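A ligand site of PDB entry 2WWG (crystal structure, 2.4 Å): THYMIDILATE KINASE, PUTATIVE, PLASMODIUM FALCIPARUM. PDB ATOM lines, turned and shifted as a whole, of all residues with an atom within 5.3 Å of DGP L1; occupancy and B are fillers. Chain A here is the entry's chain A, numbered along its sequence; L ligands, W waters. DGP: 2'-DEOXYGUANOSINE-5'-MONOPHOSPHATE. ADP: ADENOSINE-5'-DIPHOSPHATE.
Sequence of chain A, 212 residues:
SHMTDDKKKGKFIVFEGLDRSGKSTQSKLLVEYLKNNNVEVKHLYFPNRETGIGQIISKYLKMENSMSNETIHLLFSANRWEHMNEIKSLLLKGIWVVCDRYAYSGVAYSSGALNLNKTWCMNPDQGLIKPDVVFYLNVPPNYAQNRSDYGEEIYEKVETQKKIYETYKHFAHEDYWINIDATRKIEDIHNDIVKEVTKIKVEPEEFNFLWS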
ATOM      1  N   ASP A  19      17.996  -6.341  23.799  1.00  0.00           N
ATOM      2  CA  ASP A  19      17.736  -7.027  25.049  1.00  0.00           C
ATOM      3  C   ASP A  19      18.789  -6.684  26.124  1.00  0.00           C
ATOM      4  O   ASP A  19      20.023  -6.687  25.855  1.00  0.00           O
ATOM      5  CB  ASP A  19      17.693  -8.524  24.781  1.00  0.00           C
ATOM      6  CG  ASP A  19      16.515  -8.892  23.856  1.00  0.00           C
ATOM      7  OD1 ASP A  19      15.448  -9.129  24.418  1.00  0.00           O
ATOM      8  OD2 ASP A  19      16.610  -8.893  22.603  1.00  0.00           O
ATOM      9  N   ARG A  20      18.255  -6.417  27.330  1.00  0.00           N
ATOM     10  CA  ARG A  20      19.024  -6.061  28.511  1.00  0.00           C
ATOM     11  C   ARG A  20      19.780  -4.726  28.317  1.00  0.00           C
ATOM     12  O   ARG A  20      20.926  -4.583  28.757  1.00  0.00           O
ATOM     13  CB  ARG A  20      20.040  -7.165  28.872  1.00  0.00           C
ATOM     14  CG  ARG A  20      19.537  -8.572  29.158  1.00  0.00           C
ATOM     15  CD  ARG A  20      18.270  -8.615  29.914  1.00  0.00           C
ATOM     16  NE  ARG A  20      18.217  -9.775  30.807  1.00  0.00           N
ATOM     17  CZ  ARG A  20      17.530 -10.894  30.594  1.00  0.00           C
ATOM     18  NH1 ARG A  20      16.821 -11.067  29.496  1.00  0.00           N
ATOM     19  NH2 ARG A  20      17.564 -11.829  31.500  1.00  0.00           N
ATOM     20  N   LYS A  23      16.065  -0.668  29.418  1.00  0.00           N
ATOM     21  CA  LYS A  23      14.667  -0.142  29.193  1.00  0.00           C
ATOM     22  C   LYS A  23      13.889  -0.075  30.480  1.00  0.00           C
ATOM     23  O   LYS A  23      13.353   0.988  30.841  1.00  0.00           O
ATOM     24  CB  LYS A  23      13.910  -0.992  28.150  1.00  0.00           C
ATOM     25  CG  LYS A  23      14.495  -0.783  26.739  1.00  0.00           C
ATOM     26  CD  LYS A  23      13.745  -1.463  25.649  1.00  0.00           C
ATOM     27  CE  LYS A  23      14.210  -2.867  25.373  1.00  0.00           C
ATOM     28  NZ  LYS A  23      14.418  -3.797  26.473  1.00  0.00           N
ATOM     29  N   PHE A  46       5.397  -4.126  26.614  1.00  0.00           N
ATOM     30  CA  PHE A  46       5.081  -5.144  25.688  1.00  0.00           C
ATOM     31  C   PHE A  46       6.252  -6.075  25.543  1.00  0.00           C
ATOM     32  O   PHE A  46       7.365  -5.616  25.592  1.00  0.00           O
ATOM     33  CB  PHE A  46       4.793  -4.498  24.384  1.00  0.00           C
ATOM     34  CG  PHE A  46       3.557  -3.741  24.416  1.00  0.00           C
ATOM     35  CD1 PHE A  46       2.337  -4.397  24.604  1.00  0.00           C
ATOM     36  CD2 PHE A  46       3.595  -2.355  24.355  1.00  0.00           C
ATOM     37  CE1 PHE A  46       1.175  -3.683  24.690  1.00  0.00           C
ATOM     38  CE2 PHE A  46       2.410  -1.640  24.402  1.00  0.00           C
ATOM     39  CZ  PHE A  46       1.223  -2.286  24.583  1.00  0.00           C
ATOM     40  N   PRO A  47       5.997  -7.382  25.372  1.00  0.00           N
ATOM     41  CA  PRO A  47       4.632  -7.940  25.399  1.00  0.00           C
ATOM     42  C   PRO A  47       4.161  -7.966  26.816  1.00  0.00           C
ATOM     43  O   PRO A  47       4.976  -8.110  27.752  1.00  0.00           O
ATOM     44  CB  PRO A  47       4.825  -9.402  24.951  1.00  0.00           C
ATOM     45  CG  PRO A  47       6.224  -9.719  25.419  1.00  0.00           C
ATOM     46  CD  PRO A  47       7.014  -8.429  25.223  1.00  0.00           C
ATOM     47  N   ARG A  49       2.757 -10.306  29.083  1.00  0.00           N
ATOM     48  CA  ARG A  49       2.716 -11.759  29.149  1.00  0.00           C
ATOM     49  C   ARG A  49       1.581 -12.336  29.998  1.00  0.00           C
ATOM     50  O   ARG A  49       1.476 -13.552  30.102  1.00  0.00           O
ATOM     51  CB  ARG A  49       4.055 -12.342  29.580  1.00  0.00           C
ATOM     52  CG  ARG A  49       5.233 -11.857  28.712  1.00  0.00           C
ATOM     53  CD  ARG A  49       6.522 -12.202  29.475  1.00  0.00           C
ATOM     54  NE  ARG A  49       7.802 -11.782  28.886  1.00  0.00           N
ATOM     55  CZ  ARG A  49       8.806 -12.636  28.657  1.00  0.00           C
ATOM     56  NH1 ARG A  49       8.652 -13.943  28.914  1.00  0.00           N
ATOM     57  NH2 ARG A  49       9.948 -12.205  28.184  1.00  0.00           N
ATOM     58  N   LEU A  61       8.998 -17.228  23.892  1.00  0.00           N
ATOM     59  CA  LEU A  61      10.278 -16.600  24.233  1.00  0.00           C
ATOM     60  C   LEU A  61      11.136 -17.505  25.098  1.00  0.00           C
ATOM     61  O   LEU A  61      12.372 -17.451  25.043  1.00  0.00           O
ATOM     62  CB  LEU A  61      10.038 -15.267  24.938  1.00  0.00           C
ATOM     63  CG  LEU A  61       9.409 -14.193  24.032  1.00  0.00           C
ATOM     64  CD1 LEU A  61       8.908 -13.022  24.866  1.00  0.00           C
ATOM     65  CD2 LEU A  61      10.347 -13.736  22.870  1.00  0.00           C
ATOM     66  N   ILE A  72       3.879 -15.873  15.301  1.00  0.00           N
ATOM     67  CA  ILE A  72       4.366 -15.181  16.467  1.00  0.00           C
ATOM     68  C   ILE A  72       4.322 -13.653  16.232  1.00  0.00           C
ATOM     69  O   ILE A  72       3.821 -12.936  17.077  1.00  0.00           O
ATOM     70  CB  ILE A  72       5.761 -15.701  16.942  1.00  0.00           C
ATOM     71  CG1 ILE A  72       6.042 -15.184  18.332  1.00  0.00           C
ATOM     72  CG2 ILE A  72       6.838 -15.315  16.039  1.00  0.00           C
ATOM     73  CD1 ILE A  72       5.039 -15.618  19.417  1.00  0.00           C
ATOM     74  N   HIS A  73       4.683 -13.187  15.029  1.00  0.00           N
ATOM     75  CA  HIS A  73       4.555 -11.734  14.745  1.00  0.00           C
ATOM     76  C   HIS A  73       3.144 -11.217  14.942  1.00  0.00           C
ATOM     77  O   HIS A  73       2.933 -10.125  15.455  1.00  0.00           O
ATOM     78  CB  HIS A  73       5.070 -11.345  13.350  1.00  0.00           C
ATOM     79  CG  HIS A  73       4.931  -9.865  13.078  1.00  0.00           C
ATOM     80  ND1 HIS A  73       5.618  -8.903  13.784  1.00  0.00           N
ATOM     81  CD2 HIS A  73       4.124  -9.200  12.210  1.00  0.00           C
ATOM     82  CE1 HIS A  73       5.224  -7.714  13.375  1.00  0.00           C
ATOM     83  NE2 HIS A  73       4.347  -7.865  12.407  1.00  0.00           N
ATOM     84  N   PHE A  76       2.274 -10.917  18.587  1.00  0.00           N
ATOM     85  CA  PHE A  76       2.836  -9.734  19.206  1.00  0.00           C
ATOM     86  C   PHE A  76       2.029  -8.528  18.892  1.00  0.00           C
ATOM     87  O   PHE A  76       1.782  -7.726  19.783  1.00  0.00           O
ATOM     88  CB  PHE A  76       4.235  -9.449  18.702  1.00  0.00           C
ATOM     89  CG  PHE A  76       5.284 -10.133  19.466  1.00  0.00           C
ATOM     90  CD1 PHE A  76       5.563  -9.752  20.822  1.00  0.00           C
ATOM     91  CD2 PHE A  76       6.022 -11.149  18.852  1.00  0.00           C
ATOM     92  CE1 PHE A  76       6.584 -10.403  21.569  1.00  0.00           C
ATOM     93  CE2 PHE A  76       7.081 -11.815  19.591  1.00  0.00           C
ATOM     94  CZ  PHE A  76       7.381 -11.427  20.958  1.00  0.00           C
ATOM     95  N   SER A  77       1.597  -8.409  17.642  1.00  0.00           N
ATOM     96  CA  SER A  77       0.778  -7.306  17.197  1.00  0.00           C
ATOM     97  C   SER A  77      -0.600  -7.324  17.814  1.00  0.00           C
ATOM     98  O   SER A  77      -1.092  -6.293  18.260  1.00  0.00           O
ATOM     99  CB  SER A  77       0.640  -7.366  15.677  1.00  0.00           C
ATOM    100  OG  SER A  77      -0.026  -6.224  15.253  1.00  0.00           O
ATOM    101  N   ARG A  80      -0.212  -6.049  21.297  1.00  0.00           N
ATOM    102  CA  ARG A  80      -0.231  -4.581  21.234  1.00  0.00           C
ATOM    103  C   ARG A  80      -1.675  -4.079  21.155  1.00  0.00           C
ATOM    104  O   ARG A  80      -2.088  -3.245  21.973  1.00  0.00           O
ATOM    105  CB  ARG A  80       0.652  -4.033  20.109  1.00  0.00           C
ATOM    106  CG  ARG A  80       2.148  -4.202  20.405  1.00  0.00           C
ATOM    107  CD  ARG A  80       3.073  -3.586  19.347  1.00  0.00           C
ATOM    108  NE  ARG A  80       3.219  -4.356  18.103  1.00  0.00           N
ATOM    109  CZ  ARG A  80       4.086  -5.367  17.933  1.00  0.00           C
ATOM    110  NH1 ARG A  80       4.867  -5.740  18.924  1.00  0.00           N
ATOM    111  NH2 ARG A  80       4.161  -6.025  16.780  1.00  0.00           N
ATOM    112  N   ARG A 101       8.988  -0.977  25.053  1.00  0.00           N
ATOM    113  CA  ARG A 101       8.717  -1.655  23.800  1.00  0.00           C
ATOM    114  C   ARG A 101       7.404  -1.237  23.206  1.00  0.00           C
ATOM    115  O   ARG A 101       6.431  -1.022  23.931  1.00  0.00           O
ATOM    116  CB  ARG A 101       8.862  -3.179  23.910  1.00  0.00           C
ATOM    117  CG  ARG A 101      10.259  -3.611  24.280  1.00  0.00           C
ATOM    118  CD  ARG A 101      10.508  -5.043  23.748  1.00  0.00           C
ATOM    119  NE  ARG A 101      11.792  -5.605  24.141  1.00  0.00           N
ATOM    120  CZ  ARG A 101      12.923  -5.448  23.478  1.00  0.00           C
ATOM    121  NH1 ARG A 101      12.970  -4.738  22.331  1.00  0.00           N
ATOM    122  NH2 ARG A 101      14.016  -6.003  23.950  1.00  0.00           N
ATOM    123  N   TYR A 102       7.416  -1.101  21.870  1.00  0.00           N
ATOM    124  CA  TYR A 102       6.249  -0.948  21.084  1.00  0.00           C
ATOM    125  C   TYR A 102       6.397  -1.592  19.701  1.00  0.00           C
ATOM    126  O   TYR A 102       7.173  -2.486  19.525  1.00  0.00           O
ATOM    127  CB  TYR A 102       5.971   0.559  20.976  1.00  0.00           C
ATOM    128  CG  TYR A 102       4.518   0.986  20.759  1.00  0.00           C
ATOM    129  CD1 TYR A 102       3.506   0.528  21.601  1.00  0.00           C
ATOM    130  CD2 TYR A 102       4.188   1.843  19.723  1.00  0.00           C
ATOM    131  CE1 TYR A 102       2.207   0.941  21.411  1.00  0.00           C
ATOM    132  CE2 TYR A 102       2.862   2.235  19.522  1.00  0.00           C
ATOM    133  CZ  TYR A 102       1.901   1.781  20.368  1.00  0.00           C
ATOM    134  OH  TYR A 102       0.594   2.197  20.190  1.00  0.00           O
ATOM    135  N   SER A 105       9.675  -2.532  17.950  1.00  0.00           N
ATOM    136  CA  SER A 105      10.113  -3.892  18.275  1.00  0.00           C
ATOM    137  C   SER A 105       9.600  -4.927  17.220  1.00  0.00           C
ATOM    138  O   SER A 105      10.333  -5.839  16.838  1.00  0.00           O
ATOM    139  CB  SER A 105       9.631  -4.308  19.664  1.00  0.00           C
ATOM    140  OG  SER A 105      10.491  -3.809  20.661  1.00  0.00           O
ATOM    141  N   GLY A 106       8.377  -4.739  16.720  1.00  0.00           N
ATOM    142  CA  GLY A 106       7.848  -5.625  15.677  1.00  0.00           C
ATOM    143  C   GLY A 106       8.758  -5.725  14.476  1.00  0.00           C
ATOM    144  O   GLY A 106       9.003  -6.807  13.973  1.00  0.00           O
ATOM    145  N   TYR A 109      12.572  -6.937  15.594  1.00  0.00           N
ATOM    146  CA  TYR A 109      12.610  -8.363  15.876  1.00  0.00           C
ATOM    147  C   TYR A 109      12.025  -9.236  14.755  1.00  0.00           C
ATOM    148  O   TYR A 109      12.642 -10.240  14.344  1.00  0.00           O
ATOM    149  CB  TYR A 109      12.008  -8.658  17.265  1.00  0.00           C
ATOM    150  CG  TYR A 109      12.932  -8.203  18.386  1.00  0.00           C
ATOM    151  CD1 TYR A 109      13.676  -9.112  19.101  1.00  0.00           C
ATOM    152  CD2 TYR A 109      13.056  -6.843  18.703  1.00  0.00           C
ATOM    153  CE1 TYR A 109      14.510  -8.724  20.094  1.00  0.00           C
ATOM    154  CE2 TYR A 109      13.915  -6.426  19.712  1.00  0.00           C
ATOM    155  CZ  TYR A 109      14.654  -7.357  20.387  1.00  0.00           C
ATOM    156  OH  TYR A 109      15.475  -6.971  21.398  1.00  0.00           O
ATOM    157  N   SER A 110      10.874  -8.871  14.228  1.00  0.00           N
ATOM    158  CA  SER A 110      10.264  -9.853  13.271  1.00  0.00           C
ATOM    159  C   SER A 110      11.020  -9.791  11.955  1.00  0.00           C
ATOM    160  O   SER A 110      11.347 -10.830  11.356  1.00  0.00           O
ATOM    161  CB  SER A 110       8.751  -9.675  13.097  1.00  0.00           C
ATOM    162  OG  SER A 110       8.025  -9.963  14.301  1.00  0.00           O
ATOM    163  N   LEU A 114      13.730 -12.824  12.476  1.00  0.00           N
ATOM    164  CA  LEU A 114      12.900 -13.851  11.853  1.00  0.00           C
ATOM    165  C   LEU A 114      12.826 -13.624  10.359  1.00  0.00           C
ATOM    166  O   LEU A 114      12.031 -14.256   9.676  1.00  0.00           O
ATOM    167  CB  LEU A 114      11.503 -13.801  12.459  1.00  0.00           C
ATOM    168  CG  LEU A 114      11.301 -13.952  13.973  1.00  0.00           C
ATOM    169  CD1 LEU A 114       9.834 -13.866  14.294  1.00  0.00           C
ATOM    170  CD2 LEU A 114      11.906 -15.266  14.487  1.00  0.00           C
ATOM    171  N   GLU A 153      16.317 -16.080  27.136  1.00  0.00           N
ATOM    172  CA  GLU A 153      15.236 -16.122  26.155  1.00  0.00           C
ATOM    173  C   GLU A 153      15.742 -16.148  24.731  1.00  0.00           C
ATOM    174  O   GLU A 153      16.947 -15.957  24.480  1.00  0.00           O
ATOM    175  CB  GLU A 153      14.151 -15.063  26.428  1.00  0.00           C
ATOM    176  CG  GLU A 153      13.402 -15.347  27.760  1.00  0.00           C
ATOM    177  CD  GLU A 153      12.326 -14.328  28.090  1.00  0.00           C
ATOM    178  OE1 GLU A 153      12.115 -13.359  27.331  1.00  0.00           O
ATOM    179  OE2 GLU A 153      11.635 -14.489  29.107  1.00  0.00           O
ATOM    180  N   TYR A 155      15.887 -14.632  21.763  1.00  0.00           N
ATOM    181  CA  TYR A 155      16.688 -13.761  20.879  1.00  0.00           C
ATOM    182  C   TYR A 155      18.057 -13.314  21.435  1.00  0.00           C
ATOM    183  O   TYR A 155      18.760 -12.506  20.828  1.00  0.00           O
ATOM    184  CB  TYR A 155      15.892 -12.552  20.513  1.00  0.00           C
ATOM    185  CG  TYR A 155      14.623 -12.858  19.813  1.00  0.00           C
ATOM    186  CD1 TYR A 155      14.596 -13.651  18.642  1.00  0.00           C
ATOM    187  CD2 TYR A 155      13.387 -12.327  20.279  1.00  0.00           C
ATOM    188  CE1 TYR A 155      13.359 -13.885  17.952  1.00  0.00           C
ATOM    189  CE2 TYR A 155      12.190 -12.539  19.599  1.00  0.00           C
ATOM    190  CZ  TYR A 155      12.193 -13.328  18.460  1.00  0.00           C
ATOM    191  OH  TYR A 155      11.028 -13.535  17.865  1.00  0.00           O
ATOM    192  N   GLU A 156      18.435 -13.846  22.596  1.00  0.00           N
ATOM    193  CA  GLU A 156      19.592 -13.315  23.342  1.00  0.00           C
ATOM    194  C   GLU A 156      20.854 -14.094  23.037  1.00  0.00           C
ATOM    195  O   GLU A 156      21.334 -14.893  23.846  1.00  0.00           O
ATOM    196  CB  GLU A 156      19.285 -13.266  24.819  1.00  0.00           C
ATOM    197  CG  GLU A 156      18.060 -12.403  25.100  1.00  0.00           C
ATOM    198  CD  GLU A 156      17.684 -12.427  26.546  1.00  0.00           C
ATOM    199  OE1 GLU A 156      18.420 -13.028  27.331  1.00  0.00           O
ATOM    200  OE2 GLU A 156      16.666 -11.845  26.926  1.00  0.00           O
HETATM  201  P   DGP L   1      11.475  -8.246  27.025  1.00  0.00           P
HETATM  202  OP1 DGP L   1      10.261  -7.716  27.906  1.00  0.00           O
HETATM  203  OP2 DGP L   1      11.916  -6.945  26.309  1.00  0.00           O
HETATM  204  OP3 DGP L   1      12.485  -8.838  27.877  1.00  0.00           O
HETATM  205  O5' DGP L   1      10.689  -9.030  25.747  1.00  0.00           O
HETATM  206  C5' DGP L   1      11.101 -10.181  25.334  1.00  0.00           C
HETATM  207  C4' DGP L   1      11.335 -10.187  23.836  1.00  0.00           C
HETATM  208  O4' DGP L   1      10.185 -10.010  23.021  1.00  0.00           O
HETATM  209  C3' DGP L   1      12.373  -9.203  23.316  1.00  0.00           C
HETATM  210  O3' DGP L   1      13.359 -10.144  22.881  1.00  0.00           O
HETATM  211  C2' DGP L   1      11.781  -8.551  22.108  1.00  0.00           C
HETATM  212  C1' DGP L   1      10.728  -9.631  21.728  1.00  0.00           C
HETATM  213  N9  DGP L   1       9.673  -8.936  21.016  1.00  0.00           N
HETATM  214  C8  DGP L   1       8.931  -7.898  21.481  1.00  0.00           C
HETATM  215  N7  DGP L   1       8.105  -7.508  20.510  1.00  0.00           N
HETATM  216  C5  DGP L   1       8.276  -8.300  19.438  1.00  0.00           C
HETATM  217  C6  DGP L   1       7.670  -8.349  18.185  1.00  0.00           C
HETATM  218  O6  DGP L   1       6.746  -7.582  17.878  1.00  0.00           O
HETATM  219  N1  DGP L   1       8.127  -9.262  17.278  1.00  0.00           N
HETATM  220  C2  DGP L   1       9.141 -10.176  17.633  1.00  0.00           C
HETATM  221  N2  DGP L   1       9.558 -11.104  16.740  1.00  0.00           N
HETATM  222  N3  DGP L   1       9.696 -10.123  18.871  1.00  0.00           N
HETATM  223  C4  DGP L   1       9.281  -9.211  19.753  1.00  0.00           C
HETATM  224  PB  ADP L   2      15.837  -4.280  29.715  1.00  0.00           P
HETATM  225  O1B ADP L   2      15.681  -5.791  29.584  1.00  0.00           O
HETATM  226  O2B ADP L   2      14.467  -3.804  30.181  1.00  0.00           O
HETATM  227  O3B ADP L   2      16.191  -3.744  28.431  1.00  0.00           O
HETATM  228  PA  ADP L   2      16.907  -3.875  32.338  1.00  0.00           P
HETATM  229  O1A ADP L   2      16.035  -5.058  32.971  1.00  0.00           O
HETATM  230  O2A ADP L   2      16.328  -2.531  32.713  1.00  0.00           O
HETATM  231  O3A ADP L   2      17.006  -4.043  30.767  1.00  0.00           O
HETATM  232  O5' ADP L   2      18.374  -4.136  32.757  1.00  0.00           O
HETATM  233  C5' ADP L   2      19.142  -5.236  32.332  1.00  0.00           C
HETATM  234  C4' ADP L   2      20.205  -5.540  33.447  1.00  0.00           C
HETATM  235  O4' ADP L   2      21.400  -4.621  33.422  1.00  0.00           O
HETATM  236  C3' ADP L   2      19.607  -5.343  34.858  1.00  0.00           C
HETATM  237  O3' ADP L   2      20.321  -6.122  35.800  1.00  0.00           O
HETATM  238  C2' ADP L   2      19.916  -3.850  35.125  1.00  0.00           C
HETATM  239  O2' ADP L   2      20.076  -3.665  36.493  1.00  0.00           O
HETATM  240  C1' ADP L   2      21.280  -3.689  34.531  1.00  0.00           C
HETATM  241  N9  ADP L   2      21.529  -2.349  33.987  1.00  0.00           N
HETATM  242  C8  ADP L   2      20.676  -1.556  33.312  1.00  0.00           C
HETATM  243  N7  ADP L   2      21.280  -0.438  32.981  1.00  0.00           N
HETATM  244  C5  ADP L   2      22.532  -0.518  33.422  1.00  0.00           C
HETATM  245  C6  ADP L   2      23.609   0.362  33.362  1.00  0.00           C
HETATM  246  N6  ADP L   2      23.462   1.551  32.704  1.00  0.00           N
HETATM  247  N1  ADP L   2      24.783  -0.032  33.951  1.00  0.00           N
HETATM  248  C2  ADP L   2      24.902  -1.180  34.599  1.00  0.00           C
HETATM  249  N3  ADP L   2      23.873  -2.040  34.674  1.00  0.00           N
HETATM  250  C4  ADP L   2      22.695  -1.712  34.073  1.00  0.00           C
HETATM  251  O   HOH W   1      14.920  -6.295  27.235  1.00  0.00           O
HETATM  252  O   HOH W   2      12.155  -4.546  27.747  1.00  0.00           O
HETATM  253  O   HOH W   3       7.658  -8.847  28.487  1.00  0.00           O
HETATM  254  O   HOH W   4      13.839 -11.459  27.083  1.00  0.00           O
HETATM  255  O   HOH W   5      13.958 -10.169  29.504  1.00  0.00           O
HETATM  256  O   HOH W   6       9.056  -5.354  27.728  1.00  0.00           O
HETATM  257  O   HOH W   7      12.965  -6.994  30.107  1.00  0.00           O
HETATM  258  O   HOH W   8      14.357 -12.821  23.821  1.00  0.00           O
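Residues that only touch DGP L1: Pro 47 (3.8 Å), Arg 49 (3.7 Å), Leu 61 (3.6 Å), Phe 76 (3.2 Å), Ser 105 (3.6 Å), Tyr 109 (3.2 Å), Leu 114 (3.7 Å) and Glu 153 (3.9 Å).
Hydrophobic or aromatic side chains that line DGP L1: Pro 47, Leu 61, Phe 76, Tyr 109, Leu 114 and Tyr 155.
The nearest printed residue that does not touch DGP L1 is Lys 23 (4.02 Å).
NE of Arg 101 is in salt-bridge range of OP2 of DGP L1.
An oxygen (O3') of DGP L1 sits at hydrogen-bond distance from the side-chain carboxylate (OD1) of Asp 19 (2.8 Å).
NH1 of Arg 80 lies within hydrogen-bond range of O6 of DGP L1.
OH of Tyr 155 sits at hydrogen-bond distance from N2 of DGP L1.
The side-chain hydroxyl (OG) of Ser 110 sits at hydrogen-bond distance from a nitrogen (N1) of DGP L1.
The backbone NH (N) of Gly 106 lies close to an oxygen (O6) of DGP L1 (3.5 Å).
N of Lys 23 lies within hydrogen-bond range of O3B of ADP L2, 3.2 Å away.
An oxygen (O3B) of ADP L2 is in salt-bridge range of the side-chain amino group (NZ) of Lys 23.
An oxygen (O1B) of ADP L2 lies within hydrogen-bond range of the backbone NH of Arg 20, at 3.5 Å.
NH2 of Arg 101 is in salt-bridge range of OD1 of Asp 19 (3.5 Å).
The guanidinium group of Arg 101 is in hydrogen-bond range of the side-chain hydroxyl of Tyr 109 (3.1 Å).
The guanidinium group of Arg 101 lies within hydrogen-bond range of the side-chain hydroxyl of Ser 105.
OD2 of Asp 19 is in hydrogen-bond range of OH of Tyr 109.
O of Gly 106 lies close to OG of Ser 110 (3.3 Å).
A ring nitrogen (ND1) of His 73 is in hydrogen-bond range of the side-chain hydroxyl of Ser 110 (2.7 Å).
The backbone carbonyl oxygen of Tyr 109 sits at hydrogen-bond distance from the backbone NH of Leu 114 (3.4 Å).
NH2 of Arg 49 lies within salt-bridge range of OE1 of Glu 153 (2.6 Å).
Water W5 lies within hydrogen-bond range of an oxygen (OP3) of DGP L1 (2.6 Å) and the guanidinium group (NH1) of Arg 20 (3.0 Å).
Water W6 lies within hydrogen-bond range of OP1 of DGP L1 and O of Phe 46.
Water W2 lies within hydrogen-bond range of the side-chain amino group (NZ) of Lys 23, an oxygen (OP2) of DGP L1 and an oxygen (O2B) of ADP L2.
Water W3 lies within hydrogen-bond range of the backbone carbonyl oxygen (O) of Pro 47 (2.9 Å), an oxygen (OP1) of DGP L1 (2.9 Å) and the guanidinium group (NE) of Arg 49 (3.0 Å).
Water W7 lies within hydrogen-bond range of an oxygen (OP3) of DGP L1 (2.9 Å) and an oxygen (O1B) of ADP L2 (3.0 Å).
Water W8 lies within hydrogen-bond range of an oxygen (O3') of DGP L1 (3.0 Å) and the backbone NH of Tyr 155 (3.1 Å).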
